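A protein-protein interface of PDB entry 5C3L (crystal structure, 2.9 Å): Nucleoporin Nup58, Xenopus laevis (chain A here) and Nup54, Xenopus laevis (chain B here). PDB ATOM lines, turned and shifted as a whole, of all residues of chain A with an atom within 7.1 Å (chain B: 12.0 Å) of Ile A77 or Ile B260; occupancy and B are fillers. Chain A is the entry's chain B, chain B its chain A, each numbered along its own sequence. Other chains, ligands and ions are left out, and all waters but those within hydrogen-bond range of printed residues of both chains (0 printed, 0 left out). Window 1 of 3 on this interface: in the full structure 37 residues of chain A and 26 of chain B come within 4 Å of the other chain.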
ATOM      1  N   LEU A  70      22.616   6.502  -9.734  1.00  0.00           N
ATOM      2  CA  LEU A  70      24.063   6.329  -9.811  1.00  0.00           C
ATOM      3  C   LEU A  70      24.757   7.280  -8.858  1.00  0.00           C
ATOM      4  O   LEU A  70      25.770   6.937  -8.274  1.00  0.00           O
ATOM      5  CB  LEU A  70      24.585   6.551 -11.238  1.00  0.00           C
ATOM      6  CG  LEU A  70      26.051   6.154 -11.479  1.00  0.00           C
ATOM      7  CD1 LEU A  70      26.218   5.585 -12.878  1.00  0.00           C
ATOM      8  CD2 LEU A  70      27.005   7.319 -11.273  1.00  0.00           C
ATOM      9  N   ARG A  72      23.365   8.558  -6.182  1.00  0.00           N
ATOM     10  CA  ARG A  72      22.926   8.212  -4.843  1.00  0.00           C
ATOM     11  C   ARG A  72      23.870   7.182  -4.207  1.00  0.00           C
ATOM     12  O   ARG A  72      24.319   7.347  -3.059  1.00  0.00           O
ATOM     13  CB  ARG A  72      21.494   7.689  -4.887  1.00  0.00           C
ATOM     14  CG  ARG A  72      20.478   8.680  -4.357  1.00  0.00           C
ATOM     15  CD  ARG A  72      19.075   8.126  -4.431  1.00  0.00           C
ATOM     16  NE  ARG A  72      18.357   8.619  -5.598  1.00  0.00           N
ATOM     17  CZ  ARG A  72      17.844   7.861  -6.564  1.00  0.00           C
ATOM     18  NH1 ARG A  72      17.945   6.542  -6.531  1.00  0.00           N
ATOM     19  NH2 ARG A  72      17.209   8.435  -7.578  1.00  0.00           N
ATOM     20  N   ASN A  73      24.210   6.141  -4.958  1.00  0.00           N
ATOM     21  CA  ASN A  73      24.986   5.065  -4.385  1.00  0.00           C
ATOM     22  C   ASN A  73      26.485   5.212  -4.705  1.00  0.00           C
ATOM     23  O   ASN A  73      27.303   4.423  -4.233  1.00  0.00           O
ATOM     24  CB  ASN A  73      24.411   3.715  -4.852  1.00  0.00           C
ATOM     25  CG  ASN A  73      24.384   3.577  -6.342  1.00  0.00           C
ATOM     26  OD1 ASN A  73      25.194   4.170  -7.031  1.00  0.00           O
ATOM     27  ND2 ASN A  73      23.455   2.781  -6.852  1.00  0.00           N
ATOM     28  N   ALA A  74      26.845   6.236  -5.479  1.00  0.00           N
ATOM     29  CA  ALA A  74      28.248   6.647  -5.608  1.00  0.00           C
ATOM     30  C   ALA A  74      28.683   7.292  -4.297  1.00  0.00           C
ATOM     31  O   ALA A  74      29.812   7.113  -3.851  1.00  0.00           O
ATOM     32  CB  ALA A  74      28.437   7.604  -6.759  1.00  0.00           C
ATOM     33  N   LEU A  75      27.765   8.037  -3.683  1.00  0.00           N
ATOM     34  CA  LEU A  75      27.944   8.535  -2.320  1.00  0.00           C
ATOM     35  C   LEU A  75      28.078   7.387  -1.329  1.00  0.00           C
ATOM     36  O   LEU A  75      28.899   7.430  -0.416  1.00  0.00           O
ATOM     37  CB  LEU A  75      26.766   9.417  -1.900  1.00  0.00           C
ATOM     38  CG  LEU A  75      26.619  10.800  -2.534  1.00  0.00           C
ATOM     39  CD1 LEU A  75      25.519  11.576  -1.832  1.00  0.00           C
ATOM     40  CD2 LEU A  75      27.930  11.571  -2.509  1.00  0.00           C
ATOM     41  N   ALA A  76      27.243   6.372  -1.510  1.00  0.00           N
ATOM     42  CA  ALA A  76      27.246   5.191  -0.657  1.00  0.00           C
ATOM     43  C   ALA A  76      28.590   4.486  -0.731  1.00  0.00           C
ATOM     44  O   ALA A  76      29.030   3.857   0.231  1.00  0.00           O
ATOM     45  CB  ALA A  76      26.133   4.241  -1.074  1.00  0.00           C
ATOM     46  N   ILE A  77      29.241   4.610  -1.880  1.00  0.00           N
ATOM     47  CA  ILE A  77      30.459   3.875  -2.164  1.00  0.00           C
ATOM     48  C   ILE A  77      31.680   4.604  -1.623  1.00  0.00           C
ATOM     49  O   ILE A  77      32.645   3.982  -1.203  1.00  0.00           O
ATOM     50  CB  ILE A  77      30.594   3.632  -3.687  1.00  0.00           C
ATOM     51  CG1 ILE A  77      29.742   2.422  -4.075  1.00  0.00           C
ATOM     52  CG2 ILE A  77      32.056   3.416  -4.106  1.00  0.00           C
ATOM     53  CD1 ILE A  77      29.595   2.190  -5.550  1.00  0.00           C
ATOM     54  N   ASP A  78      31.650   5.921  -1.620  1.00  0.00           N
ATOM     55  CA  ASP A  78      32.801   6.636  -1.123  1.00  0.00           C
ATOM     56  C   ASP A  78      32.793   6.537   0.386  1.00  0.00           C
ATOM     57  O   ASP A  78      33.841   6.424   1.014  1.00  0.00           O
ATOM     58  CB  ASP A  78      32.805   8.093  -1.587  1.00  0.00           C
ATOM     59  CG  ASP A  78      34.207   8.609  -1.819  1.00  0.00           C
ATOM     60  OD1 ASP A  78      34.854   8.116  -2.777  1.00  0.00           O
ATOM     61  OD2 ASP A  78      34.671   9.480  -1.045  1.00  0.00           O
ATOM     62  N   LYS A  79      31.600   6.559   0.965  1.00  0.00           N
ATOM     63  CA  LYS A  79      31.467   6.468   2.409  1.00  0.00           C
ATOM     64  C   LYS A  79      32.001   5.109   2.856  1.00  0.00           C
ATOM     65  O   LYS A  79      32.671   4.986   3.871  1.00  0.00           O
ATOM     66  CB  LYS A  79      30.008   6.654   2.824  1.00  0.00           C
ATOM     67  CG  LYS A  79      29.815   6.881   4.304  1.00  0.00           C
ATOM     68  CD  LYS A  79      28.433   6.431   4.761  1.00  0.00           C
ATOM     69  CE  LYS A  79      28.360   6.319   6.283  1.00  0.00           C
ATOM     70  NZ  LYS A  79      27.117   5.653   6.776  1.00  0.00           N
ATOM     71  N   LEU A  80      31.703   4.093   2.060  1.00  0.00           N
ATOM     72  CA  LEU A  80      32.095   2.721   2.336  1.00  0.00           C
ATOM     73  C   LEU A  80      33.600   2.515   2.186  1.00  0.00           C
ATOM     74  O   LEU A  80      34.232   1.819   2.980  1.00  0.00           O
ATOM     75  CB  LEU A  80      31.339   1.798   1.387  1.00  0.00           C
ATOM     76  CG  LEU A  80      31.329   0.295   1.617  1.00  0.00           C
ATOM     77  CD1 LEU A  80      30.905  -0.048   3.039  1.00  0.00           C
ATOM     78  CD2 LEU A  80      30.385  -0.306   0.596  1.00  0.00           C
ATOM     79  N   LYS A  81      34.170   3.124   1.154  1.00  0.00           N
ATOM     80  CA  LYS A  81      35.596   3.013   0.889  1.00  0.00           C
ATOM     81  C   LYS A  81      36.390   3.620   2.035  1.00  0.00           C
ATOM     82  O   LYS A  81      37.395   3.074   2.461  1.00  0.00           O
ATOM     83  CB  LYS A  81      35.940   3.706  -0.430  1.00  0.00           C
ATOM     84  CG  LYS A  81      37.418   3.765  -0.726  1.00  0.00           C
ATOM     85  CD  LYS A  81      37.695   4.156  -2.171  1.00  0.00           C
ATOM     86  CE  LYS A  81      38.173   5.590  -2.281  1.00  0.00           C
ATOM     87  NZ  LYS A  81      38.179   6.060  -3.690  1.00  0.00           N
ATOM     88  N   ILE A  82      35.921   4.754   2.535  1.00  0.00           N
ATOM     89  CA  ILE A  82      36.601   5.464   3.609  1.00  0.00           C
ATOM     90  C   ILE A  82      36.584   4.652   4.886  1.00  0.00           C
ATOM     91  O   ILE A  82      37.598   4.519   5.569  1.00  0.00           O
ATOM     92  CB  ILE A  82      35.938   6.833   3.868  1.00  0.00           C
ATOM     93  CG1 ILE A  82      36.285   7.786   2.729  1.00  0.00           C
ATOM     94  CG2 ILE A  82      36.378   7.417   5.200  1.00  0.00           C
ATOM     95  CD1 ILE A  82      35.519   9.062   2.761  1.00  0.00           C
ATOM     96  N   GLU A  83      35.416   4.105   5.193  1.00  0.00           N
ATOM     97  CA  GLU A  83      35.202   3.358   6.422  1.00  0.00           C
ATOM     98  C   GLU A  83      35.983   2.037   6.435  1.00  0.00           C
ATOM     99  O   GLU A  83      36.556   1.665   7.463  1.00  0.00           O
ATOM    100  CB  GLU A  83      33.708   3.103   6.610  1.00  0.00           C
ATOM    101  CG  GLU A  83      32.954   4.352   6.988  1.00  0.00           C
ATOM    102  CD  GLU A  83      31.510   4.092   7.303  1.00  0.00           C
ATOM    103  OE1 GLU A  83      30.998   3.023   6.910  1.00  0.00           O
ATOM    104  OE2 GLU A  83      30.892   4.956   7.960  1.00  0.00           O
ATOM    105  N   LEU B 249      22.813  -0.716 -18.438  1.00  0.00           N
ATOM    106  CA  LEU B 249      23.017   0.211 -17.342  1.00  0.00           C
ATOM    107  C   LEU B 249      22.141  -0.112 -16.160  1.00  0.00           C
ATOM    108  O   LEU B 249      22.603  -0.182 -15.025  1.00  0.00           O
ATOM    109  CB  LEU B 249      22.727   1.625 -17.795  1.00  0.00           C
ATOM    110  CG  LEU B 249      23.609   2.678 -17.138  1.00  0.00           C
ATOM    111  CD1 LEU B 249      23.154   4.030 -17.613  1.00  0.00           C
ATOM    112  CD2 LEU B 249      23.614   2.578 -15.601  1.00  0.00           C
ATOM    113  N   GLN B 250      20.860  -0.296 -16.439  1.00  0.00           N
ATOM    114  CA  GLN B 250      19.874  -0.569 -15.410  1.00  0.00           C
ATOM    115  C   GLN B 250      20.254  -1.816 -14.650  1.00  0.00           C
ATOM    116  O   GLN B 250      20.172  -1.852 -13.426  1.00  0.00           O
ATOM    117  CB  GLN B 250      18.499  -0.710 -16.037  1.00  0.00           C
ATOM    118  CG  GLN B 250      18.002   0.604 -16.611  1.00  0.00           C
ATOM    119  CD  GLN B 250      16.605   0.528 -17.166  1.00  0.00           C
ATOM    120  OE1 GLN B 250      16.282  -0.358 -17.953  1.00  0.00           O
ATOM    121  NE2 GLN B 250      15.762   1.465 -16.754  1.00  0.00           N
ATOM    122  N   LYS B 251      20.716  -2.826 -15.376  1.00  0.00           N
ATOM    123  CA  LYS B 251      21.066  -4.088 -14.749  1.00  0.00           C
ATOM    124  C   LYS B 251      22.400  -3.898 -14.021  1.00  0.00           C
ATOM    125  O   LYS B 251      22.571  -4.373 -12.900  1.00  0.00           O
ATOM    126  CB  LYS B 251      21.110  -5.229 -15.786  1.00  0.00           C
ATOM    127  CG  LYS B 251      22.461  -5.488 -16.450  1.00  0.00           C
ATOM    128  CD  LYS B 251      22.437  -6.731 -17.354  1.00  0.00           C
ATOM    129  CE  LYS B 251      23.844  -7.335 -17.518  1.00  0.00           C
ATOM    130  NZ  LYS B 251      23.898  -8.468 -18.491  1.00  0.00           N
ATOM    131  N   ASN B 252      23.331  -3.183 -14.644  1.00  0.00           N
ATOM    132  CA  ASN B 252      24.580  -2.814 -13.983  1.00  0.00           C
ATOM    133  C   ASN B 252      24.282  -2.081 -12.685  1.00  0.00           C
ATOM    134  O   ASN B 252      24.937  -2.297 -11.670  1.00  0.00           O
ATOM    135  CB  ASN B 252      25.447  -1.939 -14.893  1.00  0.00           C
ATOM    136  CG  ASN B 252      26.110  -2.726 -16.009  1.00  0.00           C
ATOM    137  OD1 ASN B 252      25.902  -3.932 -16.141  1.00  0.00           O
ATOM    138  ND2 ASN B 252      26.915  -2.044 -16.824  1.00  0.00           N
ATOM    139  N   GLN B 253      23.267  -1.231 -12.718  1.00  0.00           N
ATOM    140  CA  GLN B 253      22.894  -0.446 -11.555  1.00  0.00           C
ATOM    141  C   GLN B 253      22.423  -1.365 -10.420  1.00  0.00           C
ATOM    142  O   GLN B 253      22.819  -1.200  -9.273  1.00  0.00           O
ATOM    143  CB  GLN B 253      21.802   0.563 -11.932  1.00  0.00           C
ATOM    144  CG  GLN B 253      21.660   1.757 -10.986  1.00  0.00           C
ATOM    145  CD  GLN B 253      20.384   2.573 -11.237  1.00  0.00           C
ATOM    146  OE1 GLN B 253      19.515   2.175 -12.019  1.00  0.00           O
ATOM    147  NE2 GLN B 253      20.276   3.722 -10.578  1.00  0.00           N
ATOM    148  N   THR B 254      21.590  -2.347 -10.752  1.00  0.00           N
ATOM    149  CA  THR B 254      20.996  -3.238  -9.749  1.00  0.00           C
ATOM    150  C   THR B 254      22.060  -4.114  -9.090  1.00  0.00           C
ATOM    151  O   THR B 254      22.014  -4.366  -7.880  1.00  0.00           O
ATOM    152  CB  THR B 254      19.911  -4.146 -10.370  1.00  0.00           C
ATOM    153  OG1 THR B 254      18.775  -3.355 -10.722  1.00  0.00           O
ATOM    154  CG2 THR B 254      19.462  -5.209  -9.388  1.00  0.00           C
ATOM    155  N   THR B 255      23.000  -4.593  -9.902  1.00  0.00           N
ATOM    156  CA  THR B 255      24.176  -5.297  -9.404  1.00  0.00           C
ATOM    157  C   THR B 255      24.953  -4.414  -8.427  1.00  0.00           C
ATOM    158  O   THR B 255      25.333  -4.850  -7.340  1.00  0.00           O
ATOM    159  CB  THR B 255      25.122  -5.724 -10.559  1.00  0.00           C
ATOM    160  OG1 THR B 255      24.486  -6.725 -11.356  1.00  0.00           O
ATOM    161  CG2 THR B 255      26.434  -6.296 -10.026  1.00  0.00           C
ATOM    162  N   THR B 256      25.185  -3.168  -8.820  1.00  0.00           N
ATOM    163  CA  THR B 256      25.976  -2.240  -8.020  1.00  0.00           C
ATOM    164  C   THR B 256      25.318  -2.015  -6.663  1.00  0.00           C
ATOM    165  O   THR B 256      25.992  -2.010  -5.631  1.00  0.00           O
ATOM    166  CB  THR B 256      26.170  -0.896  -8.765  1.00  0.00           C
ATOM    167  OG1 THR B 256      26.899  -1.137  -9.972  1.00  0.00           O
ATOM    168  CG2 THR B 256      26.960   0.100  -7.941  1.00  0.00           C
ATOM    169  N   MET B 257      24.000  -1.859  -6.658  1.00  0.00           N
ATOM    170  CA  MET B 257      23.266  -1.684  -5.408  1.00  0.00           C
ATOM    171  C   MET B 257      23.409  -2.926  -4.530  1.00  0.00           C
ATOM    172  O   MET B 257      23.426  -2.830  -3.301  1.00  0.00           O
ATOM    173  CB  MET B 257      21.790  -1.398  -5.687  1.00  0.00           C
ATOM    174  CG  MET B 257      21.539  -0.105  -6.449  1.00  0.00           C
ATOM    175  SD  MET B 257      19.793   0.175  -6.782  1.00  0.00           S
ATOM    176  CE  MET B 257      19.182   0.457  -5.127  1.00  0.00           C
ATOM    177  N   ALA B 258      23.543  -4.085  -5.171  1.00  0.00           N
ATOM    178  CA  ALA B 258      23.579  -5.363  -4.462  1.00  0.00           C
ATOM    179  C   ALA B 258      24.904  -5.534  -3.762  1.00  0.00           C
ATOM    180  O   ALA B 258      24.957  -5.918  -2.588  1.00  0.00           O
ATOM    181  CB  ALA B 258      23.341  -6.517  -5.426  1.00  0.00           C
ATOM    182  N   LYS B 259      25.974  -5.242  -4.498  1.00  0.00           N
ATOM    183  CA  LYS B 259      27.326  -5.318  -3.967  1.00  0.00           C
ATOM    184  C   LYS B 259      27.503  -4.313  -2.836  1.00  0.00           C
ATOM    185  O   LYS B 259      28.198  -4.582  -1.847  1.00  0.00           O
ATOM    186  CB  LYS B 259      28.343  -5.071  -5.070  1.00  0.00           C
ATOM    187  CG  LYS B 259      28.334  -6.149  -6.134  1.00  0.00           C
ATOM    188  CD  LYS B 259      29.564  -6.086  -7.011  1.00  0.00           C
ATOM    189  CE  LYS B 259      29.627  -7.280  -7.940  1.00  0.00           C
ATOM    190  NZ  LYS B 259      30.709  -7.135  -8.948  1.00  0.00           N
ATOM    191  N   ILE B 260      26.853  -3.161  -2.960  1.00  0.00           N
ATOM    192  CA  ILE B 260      26.895  -2.195  -1.876  1.00  0.00           C
ATOM    193  C   ILE B 260      26.297  -2.799  -0.612  1.00  0.00           C
ATOM    194  O   ILE B 260      26.871  -2.662   0.467  1.00  0.00           O
ATOM    195  CB  ILE B 260      26.170  -0.891  -2.248  1.00  0.00           C
ATOM    196  CG1 ILE B 260      27.026  -0.128  -3.257  1.00  0.00           C
ATOM    197  CG2 ILE B 260      25.927  -0.024  -1.006  1.00  0.00           C
ATOM    198  CD1 ILE B 260      26.377   1.067  -3.825  1.00  0.00           C
ATOM    199  N   GLY B 261      25.165  -3.486  -0.747  1.00  0.00           N
ATOM    200  CA  GLY B 261      24.512  -4.119   0.391  1.00  0.00           C
ATOM    201  C   GLY B 261      25.362  -5.172   1.085  1.00  0.00           C
ATOM    202  O   GLY B 261      25.421  -5.224   2.311  1.00  0.00           O
ATOM    203  N   GLN B 262      26.026  -6.013   0.296  1.00  0.00           N
ATOM    204  CA  GLN B 262      26.961  -6.984   0.843  1.00  0.00           C
ATOM    205  C   GLN B 262      28.095  -6.303   1.601  1.00  0.00           C
ATOM    206  O   GLN B 262      28.316  -6.575   2.778  1.00  0.00           O
ATOM    207  CB  GLN B 262      27.558  -7.849  -0.271  1.00  0.00           C
ATOM    208  CG  GLN B 262      26.535  -8.570  -1.122  1.00  0.00           C
ATOM    209  CD  GLN B 262      27.164  -9.350  -2.269  1.00  0.00           C
ATOM    210  OE1 GLN B 262      28.304  -9.826  -2.170  1.00  0.00           O
ATOM    211  NE2 GLN B 262      26.415  -9.481  -3.373  1.00  0.00           N
ATOM    212  N   TYR B 263      28.806  -5.414   0.914  1.00  0.00           N
ATOM    213  CA  TYR B 263      30.052  -4.868   1.432  1.00  0.00           C
ATOM    214  C   TYR B 263      29.808  -4.034   2.685  1.00  0.00           C
ATOM    215  O   TYR B 263      30.683  -3.953   3.544  1.00  0.00           O
ATOM    216  CB  TYR B 263      30.771  -4.025   0.364  1.00  0.00           C
ATOM    217  CG  TYR B 263      31.183  -4.776  -0.894  1.00  0.00           C
ATOM    218  CD1 TYR B 263      30.901  -6.123  -1.058  1.00  0.00           C
ATOM    219  CD2 TYR B 263      31.860  -4.133  -1.915  1.00  0.00           C
ATOM    220  CE1 TYR B 263      31.277  -6.804  -2.200  1.00  0.00           C
ATOM    221  CE2 TYR B 263      32.242  -4.810  -3.066  1.00  0.00           C
ATOM    222  CZ  TYR B 263      31.947  -6.151  -3.198  1.00  0.00           C
ATOM    223  OH  TYR B 263      32.319  -6.849  -4.336  1.00  0.00           O
ATOM    224  N   LYS B 264      28.634  -3.418   2.799  1.00  0.00           N
ATOM    225  CA  LYS B 264      28.282  -2.728   4.041  1.00  0.00           C
ATOM    226  C   LYS B 264      28.121  -3.768   5.147  1.00  0.00           C
ATOM    227  O   LYS B 264      28.484  -3.548   6.303  1.00  0.00           O
ATOM    228  CB  LYS B 264      26.996  -1.916   3.897  1.00  0.00           C
ATOM    229  CG  LYS B 264      27.121  -0.696   3.031  1.00  0.00           C
ATOM    230  CD  LYS B 264      26.790   0.573   3.811  1.00  0.00           C
ATOM    231  CE  LYS B 264      26.778   1.808   2.900  1.00  0.00           C
ATOM    232  NZ  LYS B 264      27.078   3.072   3.641  1.00  0.00           N
ATOM    233  N   ARG B 265      27.575  -4.913   4.768  1.00  0.00           N
ATOM    234  CA  ARG B 265      27.304  -5.973   5.710  1.00  0.00           C
ATOM    235  C   ARG B 265      28.615  -6.575   6.196  1.00  0.00           C
ATOM    236  O   ARG B 265      28.830  -6.737   7.399  1.00  0.00           O
ATOM    237  CB  ARG B 265      26.424  -7.035   5.055  1.00  0.00           C
ATOM    238  CG  ARG B 265      25.254  -7.472   5.885  1.00  0.00           C
ATOM    239  CD  ARG B 265      24.250  -8.205   5.008  1.00  0.00           C
ATOM    240  NE  ARG B 265      23.435  -7.276   4.222  1.00  0.00           N
ATOM    241  CZ  ARG B 265      23.201  -7.372   2.914  1.00  0.00           C
ATOM    242  NH1 ARG B 265      23.712  -8.361   2.186  1.00  0.00           N
ATOM    243  NH2 ARG B 265      22.443  -6.459   2.328  1.00  0.00           N
ATOM    244  N   LYS B 266      29.485  -6.914   5.254  1.00  0.00           N
ATOM    245  CA  LYS B 266      30.799  -7.441   5.594  1.00  0.00           C
ATOM    246  C   LYS B 266      31.551  -6.458   6.486  1.00  0.00           C
ATOM    247  O   LYS B 266      32.195  -6.858   7.452  1.00  0.00           O
ATOM    248  CB  LYS B 266      31.627  -7.723   4.338  1.00  0.00           C
ATOM    249  CG  LYS B 266      32.826  -8.625   4.603  1.00  0.00           C
ATOM    250  CD  LYS B 266      32.394 -10.071   4.760  1.00  0.00           C
ATOM    251  CE  LYS B 266      33.137 -10.789   5.859  1.00  0.00           C
ATOM    252  NZ  LYS B 266      32.489 -12.101   6.170  1.00  0.00           N
ATOM    253  N   LEU B 267      31.470  -5.171   6.159  1.00  0.00           N
ATOM    254  CA  LEU B 267      32.223  -4.158   6.884  1.00  0.00           C
ATOM    255  C   LEU B 267      31.746  -4.110   8.329  1.00  0.00           C
ATOM    256  O   LEU B 267      32.556  -4.029   9.270  1.00  0.00           O
ATOM    257  CB  LEU B 267      32.071  -2.788   6.224  1.00  0.00           C
ATOM    258  CG  LEU B 267      32.928  -1.684   6.846  1.00  0.00           C
ATOM    259  CD1 LEU B 267      34.418  -1.991   6.698  1.00  0.00           C
ATOM    260  CD2 LEU B 267      32.585  -0.333   6.236  1.00  0.00           C
ATOM    261  N   MET B 268      30.425  -4.179   8.483  1.00  0.00           N
ATOM    262  CA  MET B 268      29.769  -4.179   9.789  1.00  0.00           C
ATOM    263  C   MET B 268      30.235  -5.391  10.613  1.00  0.00           C
ATOM    264  O   MET B 268      30.432  -5.309  11.829  1.00  0.00           O
ATOM    265  CB  MET B 268      28.250  -4.184   9.587  1.00  0.00           C
ATOM    266  CG  MET B 268      27.397  -4.123  10.857  1.00  0.00           C
ATOM    267  SD  MET B 268      25.610  -4.079  10.526  1.00  0.00           S
ATOM    268  CE  MET B 268      25.493  -2.500   9.687  1.00  0.00           C
ATOM    269  N   GLU B 269      30.429  -6.508   9.923  1.00  0.00           N
ATOM    270  CA  GLU B 269      30.923  -7.739  10.520  1.00  0.00           C
ATOM    271  C   GLU B 269      32.378  -7.602  10.956  1.00  0.00           C
ATOM    272  O   GLU B 269      32.737  -7.858  12.112  1.00  0.00           O
ATOM    273  CB  GLU B 269      30.782  -8.876   9.512  1.00  0.00           C
ATOM    274  CG  GLU B 269      31.474 -10.153   9.884  1.00  0.00           C
ATOM    275  CD  GLU B 269      31.478 -11.146   8.747  1.00  0.00           C
ATOM    276  OE1 GLU B 269      30.623 -11.018   7.845  1.00  0.00           O
ATOM    277  OE2 GLU B 269      32.342 -12.051   8.743  1.00  0.00           O
ATOM    278  N   LEU B 270      33.215  -7.207  10.004  1.00  0.00           N
ATOM    279  CA  LEU B 270      34.640  -7.080  10.231  1.00  0.00           C
ATOM    280  C   LEU B 270      34.907  -6.039  11.302  1.00  0.00           C
ATOM    281  O   LEU B 270      35.761  -6.234  12.180  1.00  0.00           O
ATOM    282  CB  LEU B 270      35.351  -6.701   8.931  1.00  0.00           C
ATOM    283  CG  LEU B 270      35.271  -7.715   7.783  1.00  0.00           C
ATOM    284  CD1 LEU B 270      35.917  -7.160   6.537  1.00  0.00           C
ATOM    285  CD2 LEU B 270      35.921  -9.030   8.159  1.00  0.00           C
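Of the 13 printed residues of chain A, 6 touch a printed residue of chain B. Printed residues of chain A that touch a printed residue of chain B: Leu A70, Asn A73, Ile A77, Lys A79, Leu A80 and Glu A83. Hydrophobic or aromatic side chains of chain A that line the printed part of chain B: Ile A77 and Leu A80. Along chain A the printed residues that touch a printed residue of chain B span positions 70 to 83. Hydrophobic or aromatic side chains of chain B within 4 Å of the printed part of chain A: Met B257, Ile B260, Tyr B263 and Leu B267. Among the printed residues, no Asp or Glu carboxylate lies within 4 Å of a Lys or Arg side-chain nitrogen of the other chain.
Asn A73 touches two residues of chain B. No residue of chain B comes within 4 Å of Ala A74. No residue of chain B comes within 4 Å of Leu A75. Ile A77 touches just one residue of chain B: Ile B260. No residue of chain B comes within 4 Å of Asp A78. Of the printed residues of chain B, Lys A79 touches Lys B264. Of chain B, only Tyr B263 (3.7 Å), Lys B264 (3.8 Å) and Leu B267 (3.6 Å) come within 4 Å of Leu A80. No residue of chain B comes within 4 Å of Lys A81. Printed residues of chain A within 4 Å of Met B257: Asn A73. Ala B258 touches none of the printed residues of chain A. Ile B260 touches just these residues of chain A: Asn A73 and Ile A77. Printed residues of chain A within 4 Å of Lys B264: Lys A79 (3.8 Å) and Leu A80 (3.8 Å). Of the printed residues of chain A, Leu B267 touches Leu A80 (3.6 Å) and Glu A83 (3.6 Å).
The backbone carbonyl oxygen (O) of Leu A70 sits close to the side-chain amide oxygen (OD1) of Asn A73 (3.1 Å).
Leu A70 touches Gln B253. ND2 of Asn A73 touches CG of Met B257, at 3.5 Å. Asn A73 touches Ile B260. Ile B260 touches Ile A77 (CD1 to CG1, 3.6 Å). Lys A79 touches Lys B264. Leu A80 touches Tyr B263 (CD2 to CB, 3.7 Å). Lys B264 touches Leu A80 (CG to CD1, 3.8 Å). Leu A80 touches Leu B267 (CD1 to CD2, 3.6 Å). Leu B267 touches Glu A83 (CD2 to CB, 3.6 Å).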
